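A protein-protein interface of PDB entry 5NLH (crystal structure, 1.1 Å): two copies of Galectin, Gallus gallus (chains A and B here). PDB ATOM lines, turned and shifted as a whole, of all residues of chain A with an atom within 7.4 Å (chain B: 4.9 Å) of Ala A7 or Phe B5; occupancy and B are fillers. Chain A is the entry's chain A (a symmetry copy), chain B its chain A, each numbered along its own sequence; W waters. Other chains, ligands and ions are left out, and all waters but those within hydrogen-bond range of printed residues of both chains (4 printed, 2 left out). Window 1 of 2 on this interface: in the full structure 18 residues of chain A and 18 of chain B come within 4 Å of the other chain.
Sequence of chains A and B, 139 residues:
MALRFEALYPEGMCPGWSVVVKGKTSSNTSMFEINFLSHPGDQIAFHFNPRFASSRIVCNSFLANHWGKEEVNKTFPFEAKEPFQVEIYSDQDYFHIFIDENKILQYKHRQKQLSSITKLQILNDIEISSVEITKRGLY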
ATOM      1  N   LEU A   3      22.310  14.973  16.655  1.00  0.00           N
ATOM      2  CA  LEU A   3      22.175  13.610  17.129  1.00  0.00           C
ATOM      3  C   LEU A   3      23.217  13.324  18.199  1.00  0.00           C
ATOM      4  O   LEU A   3      24.414  13.513  17.961  1.00  0.00           O
ATOM      5  CB  LEU A   3      22.367  12.645  15.968  1.00  0.00           C
ATOM      6  CG  LEU A   3      22.335  11.150  16.302  1.00  0.00           C
ATOM      7  CD1 LEU A   3      20.947  10.749  16.681  1.00  0.00           C
ATOM      8  CD2 LEU A   3      22.800  10.325  15.109  1.00  0.00           C
ATOM      9  N   PHE A   5      22.851  10.223  20.212  1.00  0.00           N
ATOM     10  CA  PHE A   5      22.914   8.767  20.329  1.00  0.00           C
ATOM     11  C   PHE A   5      21.844   8.150  19.438  1.00  0.00           C
ATOM     12  O   PHE A   5      20.733   8.676  19.351  1.00  0.00           O
ATOM     13  CB  PHE A   5      22.707   8.345  21.792  1.00  0.00           C
ATOM     14  CG  PHE A   5      22.776   6.858  22.014  1.00  0.00           C
ATOM     15  CD1 PHE A   5      23.979   6.234  22.310  1.00  0.00           C
ATOM     16  CD2 PHE A   5      21.636   6.073  21.945  1.00  0.00           C
ATOM     17  CE1 PHE A   5      24.032   4.858  22.526  1.00  0.00           C
ATOM     18  CE2 PHE A   5      21.702   4.708  22.147  1.00  0.00           C
ATOM     19  CZ  PHE A   5      22.886   4.116  22.437  1.00  0.00           C
ATOM     20  N   GLU A   6      22.177   7.033  18.803  1.00  0.00           N
ATOM     21  CA  GLU A   6      21.181   6.249  18.077  1.00  0.00           C
ATOM     22  C   GLU A   6      21.463   4.783  18.309  1.00  0.00           C
ATOM     23  O   GLU A   6      22.617   4.379  18.405  1.00  0.00           O
ATOM     24  CB  GLU A   6      21.204   6.587  16.577  1.00  0.00           C
ATOM     25  CG  GLU A   6      20.340   5.719  15.659  1.00  0.00           C
ATOM     26  CD  GLU A   6      20.524   6.097  14.198  1.00  0.00           C
ATOM     27  OE1 GLU A   6      20.381   7.288  13.900  1.00  0.00           O
ATOM     28  OE2 GLU A   6      20.837   5.221  13.357  1.00  0.00           O
ATOM     29  N   ALA A   7      20.409   3.983  18.378  1.00  0.00           N
ATOM     30  CA  ALA A   7      20.545   2.537  18.433  1.00  0.00           C
ATOM     31  C   ALA A   7      19.524   1.896  17.509  1.00  0.00           C
ATOM     32  O   ALA A   7      18.431   2.422  17.310  1.00  0.00           O
ATOM     33  CB  ALA A   7      20.372   2.011  19.841  1.00  0.00           C
ATOM     34  N   LEU A   8      19.914   0.754  16.961  1.00  0.00           N
ATOM     35  CA  LEU A   8      19.094  -0.018  16.044  1.00  0.00           C
ATOM     36  C   LEU A   8      19.091  -1.461  16.517  1.00  0.00           C
ATOM     37  O   LEU A   8      20.150  -2.053  16.742  1.00  0.00           O
ATOM     38  CB  LEU A   8      19.678   0.074  14.632  1.00  0.00           C
ATOM     39  CG  LEU A   8      19.032  -0.815  13.569  1.00  0.00           C
ATOM     40  CD1 LEU A   8      17.618  -0.385  13.252  1.00  0.00           C
ATOM     41  CD2 LEU A   8      19.886  -0.815  12.316  1.00  0.00           C
ATOM     42  N   TYR A   9      17.893  -2.035  16.633  1.00  0.00           N
ATOM     43  CA  TYR A   9      17.687  -3.431  16.986  1.00  0.00           C
ATOM     44  C   TYR A   9      16.679  -3.975  15.962  1.00  0.00           C
ATOM     45  O   TYR A   9      15.477  -3.819  16.134  1.00  0.00           O
ATOM     46  CB  TYR A   9      17.175  -3.577  18.424  1.00  0.00           C
ATOM     47  CG  TYR A   9      16.969  -4.999  18.840  1.00  0.00           C
ATOM     48  CD1 TYR A   9      18.045  -5.838  19.096  1.00  0.00           C
ATOM     49  CD2 TYR A   9      15.692  -5.519  18.946  1.00  0.00           C
ATOM     50  CE1 TYR A   9      17.847  -7.151  19.446  1.00  0.00           C
ATOM     51  CE2 TYR A   9      15.484  -6.828  19.292  1.00  0.00           C
ATOM     52  CZ  TYR A   9      16.564  -7.640  19.540  1.00  0.00           C
ATOM     53  OH  TYR A   9      16.360  -8.956  19.895  1.00  0.00           O
ATOM     54  N   PRO A  10      17.175  -4.533  14.844  1.00  0.00           N
ATOM     55  CA  PRO A  10      16.282  -4.822  13.711  1.00  0.00           C
ATOM     56  C   PRO A  10      15.158  -5.806  13.980  1.00  0.00           C
ATOM     57  O   PRO A  10      14.179  -5.761  13.241  1.00  0.00           O
ATOM     58  CB  PRO A  10      17.238  -5.345  12.625  1.00  0.00           C
ATOM     59  CG  PRO A  10      18.523  -4.645  12.934  1.00  0.00           C
ATOM     60  CD  PRO A  10      18.593  -4.644  14.439  1.00  0.00           C
ATOM     61  N   GLU A  11      15.282  -6.661  14.988  1.00  0.00           N
ATOM     62  CA  GLU A  11      14.229  -7.618  15.306  1.00  0.00           C
ATOM     63  C   GLU A  11      13.038  -6.944  15.990  1.00  0.00           C
ATOM     64  O   GLU A  11      11.999  -7.580  16.131  1.00  0.00           O
ATOM     65  CB  GLU A  11      14.770  -8.751  16.195  1.00  0.00           C
ATOM     66  CG  GLU A  11      15.732  -9.732  15.504  1.00  0.00           C
ATOM     67  CD  GLU A  11      16.610 -10.556  16.490  1.00  0.00           C
ATOM     68  OE1 GLU A  11      17.692 -10.083  16.954  1.00  0.00           O
ATOM     69  OE2 GLU A  11      16.198 -11.695  16.812  1.00  0.00           O
ATOM     70  N   MET A  13      12.272  -3.630  19.072  1.00  0.00           N
ATOM     71  CA  MET A  13      12.504  -3.418  20.515  1.00  0.00           C
ATOM     72  C   MET A  13      11.233  -2.920  21.201  1.00  0.00           C
ATOM     73  O   MET A  13      11.277  -2.073  22.080  1.00  0.00           O
ATOM     74  CB  MET A  13      13.704  -2.477  20.791  1.00  0.00           C
ATOM     75  CG  MET A  13      13.595  -1.082  20.127  1.00  0.00           C
ATOM     76  SD  MET A  13      14.710   0.234  20.728  1.00  0.00           S
ATOM     77  CE  MET A  13      16.158  -0.052  19.748  1.00  0.00           C
ATOM     78  N   TRP A  17      10.356  -3.971  26.266  1.00  0.00           N
ATOM     79  CA  TRP A  17      11.727  -3.496  26.432  1.00  0.00           C
ATOM     80  C   TRP A  17      11.719  -2.220  27.243  1.00  0.00           C
ATOM     81  O   TRP A  17      10.794  -1.409  27.154  1.00  0.00           O
ATOM     82  CB  TRP A  17      12.382  -3.210  25.079  1.00  0.00           C
ATOM     83  CG  TRP A  17      12.687  -4.429  24.256  1.00  0.00           C
ATOM     84  CD1 TRP A  17      11.803  -5.232  23.602  1.00  0.00           C
ATOM     85  CD2 TRP A  17      13.981  -4.975  24.007  1.00  0.00           C
ATOM     86  NE1 TRP A  17      12.471  -6.236  22.951  1.00  0.00           N
ATOM     87  CE2 TRP A  17      13.814  -6.101  23.185  1.00  0.00           C
ATOM     88  CE3 TRP A  17      15.270  -4.607  24.387  1.00  0.00           C
ATOM     89  CZ2 TRP A  17      14.892  -6.868  22.747  1.00  0.00           C
ATOM     90  CZ3 TRP A  17      16.329  -5.360  23.958  1.00  0.00           C
ATOM     91  CH2 TRP A  17      16.140  -6.486  23.154  1.00  0.00           C
ATOM     92  N   ASN A  35      13.382   9.718  20.803  1.00  0.00           N
ATOM     93  CA  ASN A  35      12.442   9.285  19.779  1.00  0.00           C
ATOM     94  C   ASN A  35      12.576   7.802  19.517  1.00  0.00           C
ATOM     95  O   ASN A  35      13.677   7.282  19.393  1.00  0.00           O
ATOM     96  CB  ASN A  35      12.662  10.041  18.469  1.00  0.00           C
ATOM     97  CG  ASN A  35      12.450  11.528  18.603  1.00  0.00           C
ATOM     98  OD1 ASN A  35      11.549  11.983  19.300  1.00  0.00           O
ATOM     99  ND2 ASN A  35      13.295  12.310  17.930  1.00  0.00           N
ATOM    100  N   LEU A  37      11.545   5.164  16.655  1.00  0.00           N
ATOM    101  CA  LEU A  37      11.208   5.199  15.239  1.00  0.00           C
ATOM    102  C   LEU A  37      10.806   3.837  14.717  1.00  0.00           C
ATOM    103  O   LEU A  37      11.376   2.807  15.112  1.00  0.00           O
ATOM    104  CB  LEU A  37      12.401   5.665  14.413  1.00  0.00           C
ATOM    105  CG  LEU A  37      13.107   6.974  14.748  1.00  0.00           C
ATOM    106  CD1 LEU A  37      12.106   8.048  14.933  1.00  0.00           C
ATOM    107  CD2 LEU A  37      13.985   6.909  15.951  1.00  0.00           C
ATOM    108  N   THR A 118      12.207  -0.214  15.710  1.00  0.00           N
ATOM    109  CA  THR A 118      13.535  -0.807  15.719  1.00  0.00           C
ATOM    110  C   THR A 118      14.635   0.183  16.089  1.00  0.00           C
ATOM    111  O   THR A 118      15.774  -0.240  16.246  1.00  0.00           O
ATOM    112  CB  THR A 118      13.882  -1.338  14.334  1.00  0.00           C
ATOM    113  OG1 THR A 118      13.794  -0.244  13.412  1.00  0.00           O
ATOM    114  CG2 THR A 118      12.942  -2.470  13.914  1.00  0.00           C
ATOM    115  N   LYS A 119      14.319   1.476  16.208  1.00  0.00           N
ATOM    116  CA  LYS A 119      15.358   2.488  16.337  1.00  0.00           C
ATOM    117  C   LYS A 119      15.010   3.483  17.421  1.00  0.00           C
ATOM    118  O   LYS A 119      13.853   3.878  17.595  1.00  0.00           O
ATOM    119  CB  LYS A 119      15.558   3.188  14.996  1.00  0.00           C
ATOM    120  CG  LYS A 119      16.702   4.163  14.963  1.00  0.00           C
ATOM    121  CD  LYS A 119      16.807   4.900  13.635  1.00  0.00           C
ATOM    122  CE  LYS A 119      17.182   3.991  12.499  1.00  0.00           C
ATOM    123  NZ  LYS A 119      17.442   4.810  11.267  1.00  0.00           N
ATOM    124  N   LEU A 120      16.060   3.908  18.110  1.00  0.00           N
ATOM    125  CA  LEU A 120      16.026   4.897  19.169  1.00  0.00           C
ATOM    126  C   LEU A 120      16.956   6.024  18.743  1.00  0.00           C
ATOM    127  O   LEU A 120      18.081   5.747  18.336  1.00  0.00           O
ATOM    128  CB  LEU A 120      16.589   4.266  20.460  1.00  0.00           C
ATOM    129  CG  LEU A 120      16.785   5.213  21.651  1.00  0.00           C
ATOM    130  CD1 LEU A 120      15.449   5.644  22.232  1.00  0.00           C
ATOM    131  CD2 LEU A 120      17.648   4.553  22.705  1.00  0.00           C
ATOM    132  N   GLN A 121      16.522   7.282  18.849  1.00  0.00           N
ATOM    133  CA  GLN A 121      17.381   8.440  18.599  1.00  0.00           C
ATOM    134  C   GLN A 121      17.258   9.388  19.787  1.00  0.00           C
ATOM    135  O   GLN A 121      16.159   9.616  20.276  1.00  0.00           O
ATOM    136  CB  GLN A 121      17.006   9.170  17.278  1.00  0.00           C
ATOM    137  CG  GLN A 121      17.518   8.442  16.017  1.00  0.00           C
ATOM    138  CD  GLN A 121      17.467   9.246  14.716  1.00  0.00           C
ATOM    139  OE1 GLN A 121      16.650  10.134  14.544  1.00  0.00           O
ATOM    140  NE2 GLN A 121      18.348   8.907  13.785  1.00  0.00           N
ATOM    141  N   ILE A 122      18.377   9.957  20.217  1.00  0.00           N
ATOM    142  CA  ILE A 122      18.401  10.953  21.274  1.00  0.00           C
ATOM    143  C   ILE A 122      19.082  12.186  20.712  1.00  0.00           C
ATOM    144  O   ILE A 122      20.201  12.080  20.203  1.00  0.00           O
ATOM    145  CB  ILE A 122      19.167  10.432  22.514  1.00  0.00           C
ATOM    146  CG1 ILE A 122      18.598   9.090  22.981  1.00  0.00           C
ATOM    147  CG2 ILE A 122      19.174  11.495  23.619  1.00  0.00           C
ATOM    148  CD1 ILE A 122      19.357   8.450  24.129  1.00  0.00           C
ATOM    149  N   VAL A 131      23.247   4.741  28.296  1.00  0.00           N
ATOM    150  CA  VAL A 131      22.025   4.259  27.674  1.00  0.00           C
ATOM    151  C   VAL A 131      22.000   2.743  27.848  1.00  0.00           C
ATOM    152  O   VAL A 131      22.956   2.059  27.475  1.00  0.00           O
ATOM    153  CB  VAL A 131      21.922   4.600  26.169  1.00  0.00           C
ATOM    154  CG1 VAL A 131      20.587   4.079  25.610  1.00  0.00           C
ATOM    155  CG2 VAL A 131      22.043   6.101  25.962  1.00  0.00           C
ATOM    156  N   ILE A 133      19.486  -0.628  27.015  1.00  0.00           N
ATOM    157  CA  ILE A 133      18.344  -1.135  26.264  1.00  0.00           C
ATOM    158  C   ILE A 133      18.212  -2.604  26.661  1.00  0.00           C
ATOM    159  O   ILE A 133      19.098  -3.402  26.375  1.00  0.00           O
ATOM    160  CB  ILE A 133      18.571  -0.965  24.756  1.00  0.00           C
ATOM    161  CG1 ILE A 133      18.761   0.528  24.435  1.00  0.00           C
ATOM    162  CG2 ILE A 133      17.419  -1.573  23.967  1.00  0.00           C
ATOM    163  CD1 ILE A 133      19.171   0.837  23.017  1.00  0.00           C
ATOM    164  N   LEU B   3      23.069  -8.290  11.110  1.00  0.00           N
ATOM    165  CA  LEU B   3      23.186  -7.289  12.152  1.00  0.00           C
ATOM    166  C   LEU B   3      22.120  -7.512  13.212  1.00  0.00           C
ATOM    167  O   LEU B   3      20.929  -7.566  12.890  1.00  0.00           O
ATOM    168  CB  LEU B   3      23.015  -5.902  11.548  1.00  0.00           C
ATOM    169  CG  LEU B   3      23.032  -4.720  12.521  1.00  0.00           C
ATOM    170  CD1 LEU B   3      24.409  -4.540  13.071  1.00  0.00           C
ATOM    171  CD2 LEU B   3      22.588  -3.442  11.820  1.00  0.00           C
ATOM    172  N   ARG B   4      22.539  -7.636  14.468  1.00  0.00           N
ATOM    173  CA  ARG B   4      21.602  -7.802  15.574  1.00  0.00           C
ATOM    174  C   ARG B   4      21.394  -6.494  16.346  1.00  0.00           C
ATOM    175  O   ARG B   4      20.320  -6.262  16.886  1.00  0.00           O
ATOM    176  CB  ARG B   4      22.064  -8.913  16.530  1.00  0.00           C
ATOM    177  CG  ARG B   4      22.420 -10.254  15.864  1.00  0.00           C
ATOM    178  CD  ARG B   4      21.311 -10.819  14.967  1.00  0.00           C
ATOM    179  NE  ARG B   4      20.180 -11.388  15.699  1.00  0.00           N
ATOM    180  CZ  ARG B   4      20.074 -12.659  16.077  1.00  0.00           C
ATOM    181  NH1 ARG B   4      21.035 -13.526  15.800  1.00  0.00           N
ATOM    182  NH2 ARG B   4      18.983 -13.071  16.716  1.00  0.00           N
ATOM    183  N   PHE B   5      22.427  -5.656  16.417  1.00  0.00           N
ATOM    184  CA  PHE B   5      22.353  -4.409  17.177  1.00  0.00           C
ATOM    185  C   PHE B   5      23.439  -3.461  16.684  1.00  0.00           C
ATOM    186  O   PHE B   5      24.555  -3.898  16.393  1.00  0.00           O
ATOM    187  CB  PHE B   5      22.526  -4.695  18.677  1.00  0.00           C
ATOM    188  CG  PHE B   5      22.445  -3.467  19.545  1.00  0.00           C
ATOM    189  CD1 PHE B   5      21.232  -3.038  20.066  1.00  0.00           C
ATOM    190  CD2 PHE B   5      23.582  -2.742  19.863  1.00  0.00           C
ATOM    191  CE1 PHE B   5      21.168  -1.908  20.878  1.00  0.00           C
ATOM    192  CE2 PHE B   5      23.505  -1.616  20.658  1.00  0.00           C
ATOM    193  CZ  PHE B   5      22.311  -1.212  21.159  1.00  0.00           C
ATOM    194  N   GLU B   6      23.114  -2.177  16.615  1.00  0.00           N
ATOM    195  CA  GLU B   6      24.121  -1.154  16.343  1.00  0.00           C
ATOM    196  C   GLU B   6      23.827   0.050  17.206  1.00  0.00           C
ATOM    197  O   GLU B   6      22.669   0.373  17.449  1.00  0.00           O
ATOM    198  CB  GLU B   6      24.133  -0.779  14.853  1.00  0.00           C
ATOM    199  CG  GLU B   6      25.012   0.406  14.444  1.00  0.00           C
ATOM    200  CD  GLU B   6      24.862   0.729  12.966  1.00  0.00           C
ATOM    201  OE1 GLU B   6      25.018  -0.200  12.166  1.00  0.00           O
ATOM    202  OE2 GLU B   6      24.562   1.893  12.605  1.00  0.00           O
ATOM    203  N   ALA B   7      24.875   0.727  17.653  1.00  0.00           N
ATOM    204  CA  ALA B   7      24.731   1.993  18.352  1.00  0.00           C
ATOM    205  C   ALA B   7      25.767   2.977  17.838  1.00  0.00           C
ATOM    206  O   ALA B   7      26.868   2.591  17.447  1.00  0.00           O
ATOM    207  CB  ALA B   7      24.870   1.825  19.848  1.00  0.00           C
ATOM    208  N   LEU B 120      29.228   0.892  17.541  1.00  0.00           N
ATOM    209  CA  LEU B 120      29.244  -0.468  18.040  1.00  0.00           C
ATOM    210  C   LEU B 120      28.330  -1.277  17.131  1.00  0.00           C
ATOM    211  O   LEU B 120      27.213  -0.840  16.868  1.00  0.00           O
ATOM    212  CB  LEU B 120      28.650  -0.486  19.465  1.00  0.00           C
ATOM    213  CG  LEU B 120      28.434  -1.867  20.094  1.00  0.00           C
ATOM    214  CD1 LEU B 120      29.759  -2.521  20.447  1.00  0.00           C
ATOM    215  CD2 LEU B 120      27.544  -1.750  21.314  1.00  0.00           C
ATOM    216  N   GLN B 121      28.768  -2.449  16.667  1.00  0.00           N
ATOM    217  CA  GLN B 121      27.921  -3.365  15.902  1.00  0.00           C
ATOM    218  C   GLN B 121      28.022  -4.748  16.537  1.00  0.00           C
ATOM    219  O   GLN B 121      29.112  -5.178  16.893  1.00  0.00           O
ATOM    220  CB  GLN B 121      28.328  -3.422  14.402  1.00  0.00           C
ATOM    221  CG  GLN B 121      27.840  -2.200  13.595  1.00  0.00           C
ATOM    222  CD  GLN B 121      27.923  -2.330  12.072  1.00  0.00           C
ATOM    223  OE1 GLN B 121      28.748  -3.049  11.536  1.00  0.00           O
ATOM    224  NE2 GLN B 121      27.061  -1.602  11.376  1.00  0.00           N
ATOM    225  N   ILE B 122      26.898  -5.444  16.638  1.00  0.00           N
ATOM    226  CA  ILE B 122      26.856  -6.810  17.130  1.00  0.00           C
ATOM    227  C   ILE B 122      26.193  -7.653  16.058  1.00  0.00           C
ATOM    228  O   ILE B 122      25.085  -7.322  15.627  1.00  0.00           O
ATOM    229  CB  ILE B 122      26.061  -6.901  18.455  1.00  0.00           C
ATOM    230  CG1 ILE B 122      26.612  -5.918  19.491  1.00  0.00           C
ATOM    231  CG2 ILE B 122      26.034  -8.349  18.961  1.00  0.00           C
ATOM    232  CD1 ILE B 122      25.825  -5.861  20.787  1.00  0.00           C
ATOM    233  N   ILE B 128      20.210 -11.207  21.895  1.00  0.00           N
ATOM    234  CA  ILE B 128      20.520 -10.176  22.872  1.00  0.00           C
ATOM    235  C   ILE B 128      19.378  -9.988  23.866  1.00  0.00           C
ATOM    236  O   ILE B 128      18.211  -9.855  23.478  1.00  0.00           O
ATOM    237  CB  ILE B 128      20.808  -8.850  22.133  1.00  0.00           C
ATOM    238  CG1 ILE B 128      22.066  -8.991  21.269  1.00  0.00           C
ATOM    239  CG2 ILE B 128      20.939  -7.691  23.106  1.00  0.00           C
ATOM    240  CD1 ILE B 128      22.292  -7.843  20.294  1.00  0.00           C
ATOM    241  N   VAL B 131      21.826  -4.414  26.095  1.00  0.00           N
ATOM    242  CA  VAL B 131      23.059  -3.710  25.784  1.00  0.00           C
ATOM    243  C   VAL B 131      23.072  -2.435  26.624  1.00  0.00           C
ATOM    244  O   VAL B 131      22.121  -1.651  26.579  1.00  0.00           O
ATOM    245  CB  VAL B 131      23.197  -3.334  24.290  1.00  0.00           C
ATOM    246  CG1 VAL B 131      24.541  -2.624  24.056  1.00  0.00           C
ATOM    247  CG2 VAL B 131      23.087  -4.580  23.425  1.00  0.00           C
ATOM    248  N   ILE B 133      25.587   0.935  27.458  1.00  0.00           N
ATOM    249  CA  ILE B 133      26.742   1.721  27.042  1.00  0.00           C
ATOM    250  C   ILE B 133      26.858   2.852  28.063  1.00  0.00           C
ATOM    251  O   ILE B 133      25.974   3.697  28.148  1.00  0.00           O
ATOM    252  CB  ILE B 133      26.548   2.251  25.615  1.00  0.00           C
ATOM    253  CG1 ILE B 133      26.373   1.065  24.651  1.00  0.00           C
ATOM    254  CG2 ILE B 133      27.714   3.144  25.211  1.00  0.00           C
ATOM    255  CD1 ILE B 133      25.996   1.432  23.237  1.00  0.00           C
HETATM  256  O   HOH W   1      22.565   0.751  24.736  1.00  0.00           O
HETATM  257  O   HOH W   2      17.954  -7.612  16.042  1.00  0.00           O
HETATM  258  O   HOH W   3      19.826 -10.431  19.140  1.00  0.00           O
HETATM  259  O   HOH W   4      16.810 -11.084  21.596  1.00  0.00           O
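The backbone NH (N) of Leu A8 sits at hydrogen-bond distance from the backbone carbonyl oxygen (O) of Glu B6, at 2.8 Å.
N of Ile B133 lies within hydrogen-bond range of O of Val A131 (2.9 Å).
The backbone carbonyl oxygen of Val B131 is in hydrogen-bond range of the backbone NH of Ile A133 (2.9 Å).
NE of Arg B4 lies within salt-bridge range of OE1 of Glu A11 (3.1 Å).
O of Ile B122 is in hydrogen-bond range of N of Arg B4, at 2.8 Å.
The backbone carbonyl oxygen (O) of Phe A5 sits at hydrogen-bond distance from the backbone NH (N) of Ile A122 (2.8 Å).
The backbone carbonyl oxygen (O) of Ala B7 sits at hydrogen-bond distance from the backbone NH (N) of Leu B120 (2.9 Å).
The side-chain amide nitrogen (NE2) of Gln B121 is in hydrogen-bond range of the side-chain carboxylate (OE1) of Glu B6 (2.6 Å).
N of Tyr A9 is in hydrogen-bond range of O of Thr A118 (2.8 Å).
NE2 of Gln A121 lies within hydrogen-bond range of OE1 of Glu A6, at 2.6 Å.
Among the printed residues, merely in contact across the chains: Ala A7 with Glu B6 (3.2 Å), Glu A6 with Ala B7 (3.2 Å), Tyr A9 with Arg B4 (3.2 Å), Leu A8 with Phe B5 (3.3 Å), Pro A10 with Arg B4 (3.4 Å), Pro A10 with Leu B3 (3.8 Å), Leu A8 with Leu B3 (3.8 Å), Val A131 with Val B131 (3.9 Å), Trp A17 with Ile B128 (3.97 Å), Ala A7 with Phe B5 (3.99 Å) and Phe A5 with Ala B7 (3.99 Å).
Of the printed residues of chain B, Ala A7 touches Phe B5 (3.99 Å) and Glu B6 (3.2 Å).
Of the printed residues of chain A, Phe B5 touches Ala A7 (3.99 Å) and Leu A8 (3.3 Å).
Of the printed residues of chain A, Ala B7 touches Phe A5 and Glu A6.
Of the printed residues of chain A, Glu B6 touches Ala A7 (3.2 Å) and Leu A8 (2.8 Å).
Printed residues of chain B within 4 Å of Glu A11: Arg B4.
Printed residues of chain B within 4 Å of Ile A133: Val B131 (2.9 Å).
Of the printed residues of chain B, Pro A10 touches Leu B3 and Arg B4.
Thr A118 touches none of the printed residues of chain B.
Hydrophobic or aromatic side chains of chain B that line the printed part of chain A: Leu B3, Phe B5 and Ala B7.
Hydrophobic or aromatic side chains of chain A that line the printed part of chain B: Phe A5, Ala A7, Leu A8, Tyr A9, Pro A10 and Trp A17.
Among the printed residues, Asp or Glu carboxylates within 4 Å of a Lys or Arg side-chain nitrogen of the other chain: Glu A11 with Arg B4.
Phe A5 touches Ala B7, and with the chains exchanged Ala A7 touches Phe B5.
Glu A6 touches Ala B7, and with the chains exchanged Ala A7 touches Glu B6.
Val B131 touches its own counterpart, Val A131.
Val A131 touches Ile B133, and with the chains exchanged Ile A133 touches Val B131.
9 positions are printed for both chains.
Water W2 lies within hydrogen-bond range of the side-chain carboxylate (OE1) of Glu A11 and the backbone carbonyl oxygen (O) of Arg B4.
Water W4 bridges O of Ile B128 and OH of Tyr A9.
Water W3 bridges the backbone NH (N) of Ile B128 (2.9 Å) and the side-chain carboxylate (OE1) of Glu A11 (3.1 Å).
Water W1 lies within hydrogen-bond range of O of Val B131 and O of Val A131.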
